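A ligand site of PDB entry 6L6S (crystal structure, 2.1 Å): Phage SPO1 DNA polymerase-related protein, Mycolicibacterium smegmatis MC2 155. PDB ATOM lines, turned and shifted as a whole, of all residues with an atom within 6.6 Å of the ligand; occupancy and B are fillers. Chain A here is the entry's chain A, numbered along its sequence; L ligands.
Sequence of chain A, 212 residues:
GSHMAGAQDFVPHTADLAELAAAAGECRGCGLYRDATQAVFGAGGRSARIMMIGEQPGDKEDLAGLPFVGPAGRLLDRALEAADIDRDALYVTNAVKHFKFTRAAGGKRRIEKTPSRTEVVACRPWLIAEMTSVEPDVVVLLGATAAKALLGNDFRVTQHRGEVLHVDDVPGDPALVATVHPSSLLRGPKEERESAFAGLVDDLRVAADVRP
The side-chain sulfur (SG) of Cys 30 is bound to an iron atom (FE1) of the ligand.
FE3 of the ligand is bound by SG of Cys 27 (2.2 Å).
A sulfur (S1) of the ligand sits close to the indole nitrogen (NE1) of Trp 126.
The side-chain sulfur (SG) of Cys 123 is bound to an iron atom (FE4) of the ligand, 2.2 Å away.
A ring nitrogen (ND1) of His 98 binds an iron atom (FE2) of the ligand (1.9 Å).
SG of Cys 30 sits close to N of Leu 32 (3.6 Å).
The side-chain sulfur (SG) of Cys 123 sits close to the backbone carbonyl oxygen (O) of Ala 95, at 3.5 Å.
The backbone carbonyl oxygen of Ala 122 lies within hydrogen-bond range of the backbone NH of Ala 7 (3.0 Å).
The side-chain sulfur (SG) of Cys 27 sits close to the backbone NH (N) of Gly 29 (3.4 Å).
SG of Cys 123 lies close to N of Lys 97 (3.5 Å).
NE2 of His 98 is in hydrogen-bond range of N of Ala 39 (3.2 Å).
The side-chain sulfur (SG) of Cys 27 sits close to the indole nitrogen (NE1) of Trp 126, 3.4 Å away.
Residues that only touch the ligand: Ala 7 (3.9 Å), Gly 29 (3.6 Å), Lys 97 (3.8 Å) and Ala 122 (3.9 Å).
Hydrophobic or aromatic side chains that line the ligand: Ala 7, His 98 and Trp 126.
Within 4 Å of the ligand: Ala 7, Cys 27, Gly 29, Cys 30, Lys 97, His 98, Ala 122, Cys 123 and Trp 126.
The nearest printed residue that does not touch the ligand is Leu 32 (4.1 Å).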
ATOM      1  N   GLY A   6      13.221   4.591 -28.569  1.00  0.00           N
ATOM      2  CA  GLY A   6      13.582   5.788 -27.840  1.00  0.00           C
ATOM      3  C   GLY A   6      12.436   6.769 -27.649  1.00  0.00           C
ATOM      4  O   GLY A   6      11.277   6.382 -27.464  1.00  0.00           O
ATOM      5  N   ALA A   7      12.774   8.059 -27.720  1.00  0.00           N
ATOM      6  CA  ALA A   7      11.888   9.151 -27.309  1.00  0.00           C
ATOM      7  C   ALA A   7      10.764   9.434 -28.293  1.00  0.00           C
ATOM      8  O   ALA A   7      10.003  10.383 -28.046  1.00  0.00           O
ATOM      9  CB  ALA A   7      12.705  10.434 -27.133  1.00  0.00           C
ATOM     10  N   PHE A  10       7.222  10.161 -27.153  1.00  0.00           N
ATOM     11  CA  PHE A  10       7.043  11.289 -26.245  1.00  0.00           C
ATOM     12  C   PHE A  10       7.130  12.635 -26.938  1.00  0.00           C
ATOM     13  O   PHE A  10       7.038  13.666 -26.268  1.00  0.00           O
ATOM     14  CB  PHE A  10       8.088  11.263 -25.127  1.00  0.00           C
ATOM     15  CG  PHE A  10       8.098  10.014 -24.303  1.00  0.00           C
ATOM     16  CD1 PHE A  10       8.716   8.869 -24.774  1.00  0.00           C
ATOM     17  CD2 PHE A  10       7.525  10.004 -23.045  1.00  0.00           C
ATOM     18  CE1 PHE A  10       8.743   7.719 -24.012  1.00  0.00           C
ATOM     19  CE2 PHE A  10       7.553   8.859 -22.269  1.00  0.00           C
ATOM     20  CZ  PHE A  10       8.158   7.704 -22.759  1.00  0.00           C
ATOM     21  N   ALA A  24       9.407  17.273 -23.098  1.00  0.00           N
ATOM     22  CA  ALA A  24      10.700  16.672 -22.781  1.00  0.00           C
ATOM     23  C   ALA A  24      10.866  16.412 -21.285  1.00  0.00           C
ATOM     24  O   ALA A  24      11.557  15.463 -20.893  1.00  0.00           O
ATOM     25  CB  ALA A  24      11.839  17.559 -23.286  1.00  0.00           C
ATOM     26  N   GLU A  26       8.753  15.138 -19.597  1.00  0.00           N
ATOM     27  CA  GLU A  26       8.030  13.890 -19.392  1.00  0.00           C
ATOM     28  C   GLU A  26       8.675  12.704 -20.081  1.00  0.00           C
ATOM     29  O   GLU A  26       8.138  11.592 -20.011  1.00  0.00           O
ATOM     30  CB  GLU A  26       6.609  14.012 -19.941  1.00  0.00           C
ATOM     31  CG  GLU A  26       5.846  15.258 -19.529  1.00  0.00           C
ATOM     32  CD  GLU A  26       5.297  15.161 -18.147  1.00  0.00           C
ATOM     33  OE1 GLU A  26       6.103  15.222 -17.201  1.00  0.00           O
ATOM     34  OE2 GLU A  26       4.068  14.986 -18.021  1.00  0.00           O
ATOM     35  N   CYS A  27       9.790  12.909 -20.771  1.00  0.00           N
ATOM     36  CA  CYS A  27      10.383  11.856 -21.591  1.00  0.00           C
ATOM     37  C   CYS A  27      10.901  10.691 -20.742  1.00  0.00           C
ATOM     38  O   CYS A  27      11.419  10.879 -19.645  1.00  0.00           O
ATOM     39  CB  CYS A  27      11.522  12.415 -22.445  1.00  0.00           C
ATOM     40  SG  CYS A  27      11.966  11.265 -23.772  1.00  0.00           S
ATOM     41  N   ARG A  28      10.717   9.468 -21.265  1.00  0.00           N
ATOM     42  CA  ARG A  28      11.296   8.254 -20.699  1.00  0.00           C
ATOM     43  C   ARG A  28      12.065   7.457 -21.765  1.00  0.00           C
ATOM     44  O   ARG A  28      12.141   6.236 -21.670  1.00  0.00           O
ATOM     45  CB  ARG A  28      10.217   7.386 -20.067  1.00  0.00           C
ATOM     46  CG  ARG A  28       9.272   8.131 -19.152  1.00  0.00           C
ATOM     47  CD  ARG A  28       9.947   8.446 -17.846  1.00  0.00           C
ATOM     48  NE  ARG A  28       9.069   9.140 -16.917  1.00  0.00           N
ATOM     49  CZ  ARG A  28       9.124  10.446 -16.669  1.00  0.00           C
ATOM     50  NH1 ARG A  28      10.024  11.198 -17.291  1.00  0.00           N
ATOM     51  NH2 ARG A  28       8.267  10.991 -15.819  1.00  0.00           N
ATOM     52  N   GLY A  29      12.614   8.127 -22.786  1.00  0.00           N
ATOM     53  CA  GLY A  29      13.226   7.429 -23.903  1.00  0.00           C
ATOM     54  C   GLY A  29      14.525   6.714 -23.594  1.00  0.00           C
ATOM     55  O   GLY A  29      14.925   5.826 -24.358  1.00  0.00           O
ATOM     56  N   CYS A  30      15.185   7.076 -22.503  1.00  0.00           N
ATOM     57  CA  CYS A  30      16.381   6.399 -22.011  1.00  0.00           C
ATOM     58  C   CYS A  30      16.416   6.636 -20.508  1.00  0.00           C
ATOM     59  O   CYS A  30      15.493   7.234 -19.947  1.00  0.00           O
ATOM     60  CB  CYS A  30      17.655   6.887 -22.742  1.00  0.00           C
ATOM     61  SG  CYS A  30      18.373   8.479 -22.239  1.00  0.00           S
ATOM     62  N   GLY A  31      17.460   6.144 -19.835  1.00  0.00           N
ATOM     63  CA  GLY A  31      17.524   6.275 -18.379  1.00  0.00           C
ATOM     64  C   GLY A  31      18.026   7.597 -17.818  1.00  0.00           C
ATOM     65  O   GLY A  31      17.938   7.817 -16.596  1.00  0.00           O
ATOM     66  N   LEU A  32      18.472   8.525 -18.674  1.00  0.00           N
ATOM     67  CA  LEU A  32      19.129   9.718 -18.156  1.00  0.00           C
ATOM     68  C   LEU A  32      18.197  10.603 -17.353  1.00  0.00           C
ATOM     69  O   LEU A  32      18.648  11.287 -16.419  1.00  0.00           O
ATOM     70  CB  LEU A  32      19.754  10.512 -19.299  1.00  0.00           C
ATOM     71  CG  LEU A  32      20.852   9.716 -19.985  1.00  0.00           C
ATOM     72  CD1 LEU A  32      21.341  10.444 -21.223  1.00  0.00           C
ATOM     73  CD2 LEU A  32      21.944   9.371 -18.944  1.00  0.00           C
ATOM     74  N   TYR A  33      16.895  10.576 -17.650  1.00  0.00           N
ATOM     75  CA  TYR A  33      15.968  11.434 -16.919  1.00  0.00           C
ATOM     76  C   TYR A  33      16.025  11.199 -15.415  1.00  0.00           C
ATOM     77  O   TYR A  33      15.701  12.105 -14.650  1.00  0.00           O
ATOM     78  CB  TYR A  33      14.535  11.229 -17.432  1.00  0.00           C
ATOM     79  CG  TYR A  33      13.906   9.899 -17.077  1.00  0.00           C
ATOM     80  CD1 TYR A  33      14.144   8.782 -17.848  1.00  0.00           C
ATOM     81  CD2 TYR A  33      13.038   9.783 -15.988  1.00  0.00           C
ATOM     82  CE1 TYR A  33      13.566   7.554 -17.541  1.00  0.00           C
ATOM     83  CE2 TYR A  33      12.438   8.562 -15.675  1.00  0.00           C
ATOM     84  CZ  TYR A  33      12.711   7.452 -16.457  1.00  0.00           C
ATOM     85  OH  TYR A  33      12.134   6.234 -16.160  1.00  0.00           O
ATOM     86  N   ALA A  39      14.999  18.119 -17.640  1.00  0.00           N
ATOM     87  CA  ALA A  39      15.407  18.167 -19.034  1.00  0.00           C
ATOM     88  C   ALA A  39      15.861  19.577 -19.382  1.00  0.00           C
ATOM     89  O   ALA A  39      15.270  20.564 -18.920  1.00  0.00           O
ATOM     90  CB  ALA A  39      14.269  17.743 -19.965  1.00  0.00           C
ATOM     91  N   ALA A  95      22.409  17.461 -28.236  1.00  0.00           N
ATOM     92  CA  ALA A  95      21.974  16.192 -28.793  1.00  0.00           C
ATOM     93  C   ALA A  95      21.221  15.377 -27.753  1.00  0.00           C
ATOM     94  O   ALA A  95      20.298  14.636 -28.090  1.00  0.00           O
ATOM     95  CB  ALA A  95      23.177  15.420 -29.347  1.00  0.00           C
ATOM     96  N   VAL A  96      21.614  15.496 -26.484  1.00  0.00           N
ATOM     97  CA  VAL A  96      21.015  14.761 -25.382  1.00  0.00           C
ATOM     98  C   VAL A  96      20.488  15.768 -24.372  1.00  0.00           C
ATOM     99  O   VAL A  96      21.207  16.710 -24.013  1.00  0.00           O
ATOM    100  CB  VAL A  96      22.059  13.814 -24.752  1.00  0.00           C
ATOM    101  CG1 VAL A  96      21.649  13.393 -23.315  1.00  0.00           C
ATOM    102  CG2 VAL A  96      22.258  12.622 -25.640  1.00  0.00           C
ATOM    103  N   LYS A  97      19.263  15.558 -23.893  1.00  0.00           N
ATOM    104  CA  LYS A  97      18.511  16.560 -23.137  1.00  0.00           C
ATOM    105  C   LYS A  97      18.619  16.431 -21.630  1.00  0.00           C
ATOM    106  O   LYS A  97      18.181  17.347 -20.918  1.00  0.00           O
ATOM    107  CB  LYS A  97      17.021  16.487 -23.476  1.00  0.00           C
ATOM    108  CG  LYS A  97      16.684  16.655 -24.910  1.00  0.00           C
ATOM    109  CD  LYS A  97      17.390  17.799 -25.556  1.00  0.00           C
ATOM    110  CE  LYS A  97      16.611  18.277 -26.748  1.00  0.00           C
ATOM    111  NZ  LYS A  97      17.509  18.631 -27.897  1.00  0.00           N
ATOM    112  N   HIS A  98      19.152  15.332 -21.113  1.00  0.00           N
ATOM    113  CA  HIS A  98      19.351  15.157 -19.682  1.00  0.00           C
ATOM    114  C   HIS A  98      20.825  14.922 -19.387  1.00  0.00           C
ATOM    115  O   HIS A  98      21.512  14.222 -20.119  1.00  0.00           O
ATOM    116  CB  HIS A  98      18.551  13.993 -19.087  1.00  0.00           C
ATOM    117  CG  HIS A  98      17.092  14.281 -18.903  1.00  0.00           C
ATOM    118  ND1 HIS A  98      16.122  13.743 -19.719  1.00  0.00           N
ATOM    119  CD2 HIS A  98      16.436  15.022 -17.969  1.00  0.00           C
ATOM    120  CE1 HIS A  98      14.934  14.148 -19.309  1.00  0.00           C
ATOM    121  NE2 HIS A  98      15.090  14.929 -18.252  1.00  0.00           N
ATOM    122  N   PHE A  99      21.274  15.570 -18.323  1.00  0.00           N
ATOM    123  CA  PHE A  99      22.649  15.554 -17.850  1.00  0.00           C
ATOM    124  C   PHE A  99      23.074  14.153 -17.386  1.00  0.00           C
ATOM    125  O   PHE A  99      22.449  13.587 -16.485  1.00  0.00           O
ATOM    126  CB  PHE A  99      22.776  16.581 -16.723  1.00  0.00           C
ATOM    127  CG  PHE A  99      24.146  16.676 -16.092  1.00  0.00           C
ATOM    128  CD1 PHE A  99      25.283  16.645 -16.872  1.00  0.00           C
ATOM    129  CD2 PHE A  99      24.264  16.853 -14.726  1.00  0.00           C
ATOM    130  CE1 PHE A  99      26.549  16.761 -16.313  1.00  0.00           C
ATOM    131  CE2 PHE A  99      25.525  16.974 -14.125  1.00  0.00           C
ATOM    132  CZ  PHE A  99      26.674  16.940 -14.926  1.00  0.00           C
ATOM    133  N   GLU A 119      22.162   6.370 -26.069  1.00  0.00           N
ATOM    134  CA  GLU A 119      21.429   7.518 -25.552  1.00  0.00           C
ATOM    135  C   GLU A 119      21.265   8.598 -26.624  1.00  0.00           C
ATOM    136  O   GLU A 119      20.173   9.176 -26.752  1.00  0.00           O
ATOM    137  CB  GLU A 119      22.133   8.069 -24.306  1.00  0.00           C
ATOM    138  CG  GLU A 119      21.980   7.121 -23.100  1.00  0.00           C
ATOM    139  CD  GLU A 119      23.100   7.210 -22.093  1.00  0.00           C
ATOM    140  OE1 GLU A 119      22.946   6.688 -20.976  1.00  0.00           O
ATOM    141  OE2 GLU A 119      24.164   7.778 -22.415  1.00  0.00           O
ATOM    142  N   ALA A 122      18.510   7.397 -28.811  1.00  0.00           N
ATOM    143  CA  ALA A 122      17.214   7.492 -28.153  1.00  0.00           C
ATOM    144  C   ALA A 122      16.698   8.932 -28.155  1.00  0.00           C
ATOM    145  O   ALA A 122      15.514   9.175 -28.353  1.00  0.00           O
ATOM    146  CB  ALA A 122      17.284   6.954 -26.724  1.00  0.00           C
ATOM    147  N   CYS A 123      17.603   9.899 -27.947  1.00  0.00           N
ATOM    148  CA  CYS A 123      17.166  11.281 -27.768  1.00  0.00           C
ATOM    149  C   CYS A 123      17.032  12.043 -29.082  1.00  0.00           C
ATOM    150  O   CYS A 123      16.386  13.099 -29.115  1.00  0.00           O
ATOM    151  CB  CYS A 123      18.156  11.988 -26.835  1.00  0.00           C
ATOM    152  SG  CYS A 123      17.576  13.548 -26.146  1.00  0.00           S
ATOM    153  N   ARG A 124      17.488  11.471 -30.206  1.00  0.00           N
ATOM    154  CA  ARG A 124      17.517  12.244 -31.444  1.00  0.00           C
ATOM    155  C   ARG A 124      16.135  12.690 -31.926  1.00  0.00           C
ATOM    156  O   ARG A 124      16.062  13.738 -32.582  1.00  0.00           O
ATOM    157  CB  ARG A 124      18.232  11.418 -32.530  1.00  0.00           C
ATOM    158  CG  ARG A 124      18.379  12.128 -33.868  1.00  0.00           C
ATOM    159  CD  ARG A 124      19.394  11.410 -34.726  1.00  0.00           C
ATOM    160  NE  ARG A 124      19.005  10.024 -34.957  1.00  0.00           N
ATOM    161  CZ  ARG A 124      19.834   9.056 -35.332  1.00  0.00           C
ATOM    162  NH1 ARG A 124      21.125   9.317 -35.532  1.00  0.00           N
ATOM    163  NH2 ARG A 124      19.372   7.824 -35.522  1.00  0.00           N
ATOM    164  N   PRO A 125      15.012  11.983 -31.648  1.00  0.00           N
ATOM    165  CA  PRO A 125      13.698  12.522 -32.042  1.00  0.00           C
ATOM    166  C   PRO A 125      13.419  13.958 -31.586  1.00  0.00           C
ATOM    167  O   PRO A 125      12.758  14.704 -32.315  1.00  0.00           O
ATOM    168  CB  PRO A 125      12.710  11.526 -31.408  1.00  0.00           C
ATOM    169  CG  PRO A 125      13.437  10.248 -31.439  1.00  0.00           C
ATOM    170  CD  PRO A 125      14.866  10.617 -31.082  1.00  0.00           C
ATOM    171  N   TRP A 126      13.902  14.351 -30.398  1.00  0.00           N
ATOM    172  CA  TRP A 126      13.718  15.739 -29.972  1.00  0.00           C
ATOM    173  C   TRP A 126      14.479  16.689 -30.870  1.00  0.00           C
ATOM    174  O   TRP A 126      13.985  17.766 -31.231  1.00  0.00           O
ATOM    175  CB  TRP A 126      14.190  15.931 -28.527  1.00  0.00           C
ATOM    176  CG  TRP A 126      13.383  15.182 -27.544  1.00  0.00           C
ATOM    177  CD1 TRP A 126      13.784  14.105 -26.803  1.00  0.00           C
ATOM    178  CD2 TRP A 126      12.032  15.457 -27.165  1.00  0.00           C
ATOM    179  NE1 TRP A 126      12.751  13.687 -25.988  1.00  0.00           N
ATOM    180  CE2 TRP A 126      11.665  14.504 -26.184  1.00  0.00           C
ATOM    181  CE3 TRP A 126      11.094  16.425 -27.551  1.00  0.00           C
ATOM    182  CZ2 TRP A 126      10.397  14.470 -25.604  1.00  0.00           C
ATOM    183  CZ3 TRP A 126       9.826  16.395 -26.958  1.00  0.00           C
ATOM    184  CH2 TRP A 126       9.499  15.430 -25.996  1.00  0.00           C
HETATM  185 FE1  LIG L   1      16.806  10.045 -22.827  1.00  0.00          FE
HETATM  186 FE2  LIG L   1      16.180  12.721 -21.340  1.00  0.00          FE
HETATM  187 FE3  LIG L   1      14.142  11.297 -23.343  1.00  0.00          FE
HETATM  188 FE4  LIG L   1      16.666  12.499 -24.377  1.00  0.00          FE
HETATM  189  S1  LIG L   1      15.042  13.299 -23.128  1.00  0.00           S
HETATM  190  S2  LIG L   1      15.710  10.536 -24.655  1.00  0.00           S
HETATM  191  S3  LIG L   1      17.796  11.990 -22.604  1.00  0.00           S
HETATM  192  S4  LIG L   1      15.189  10.766 -21.516  1.00  0.00           S
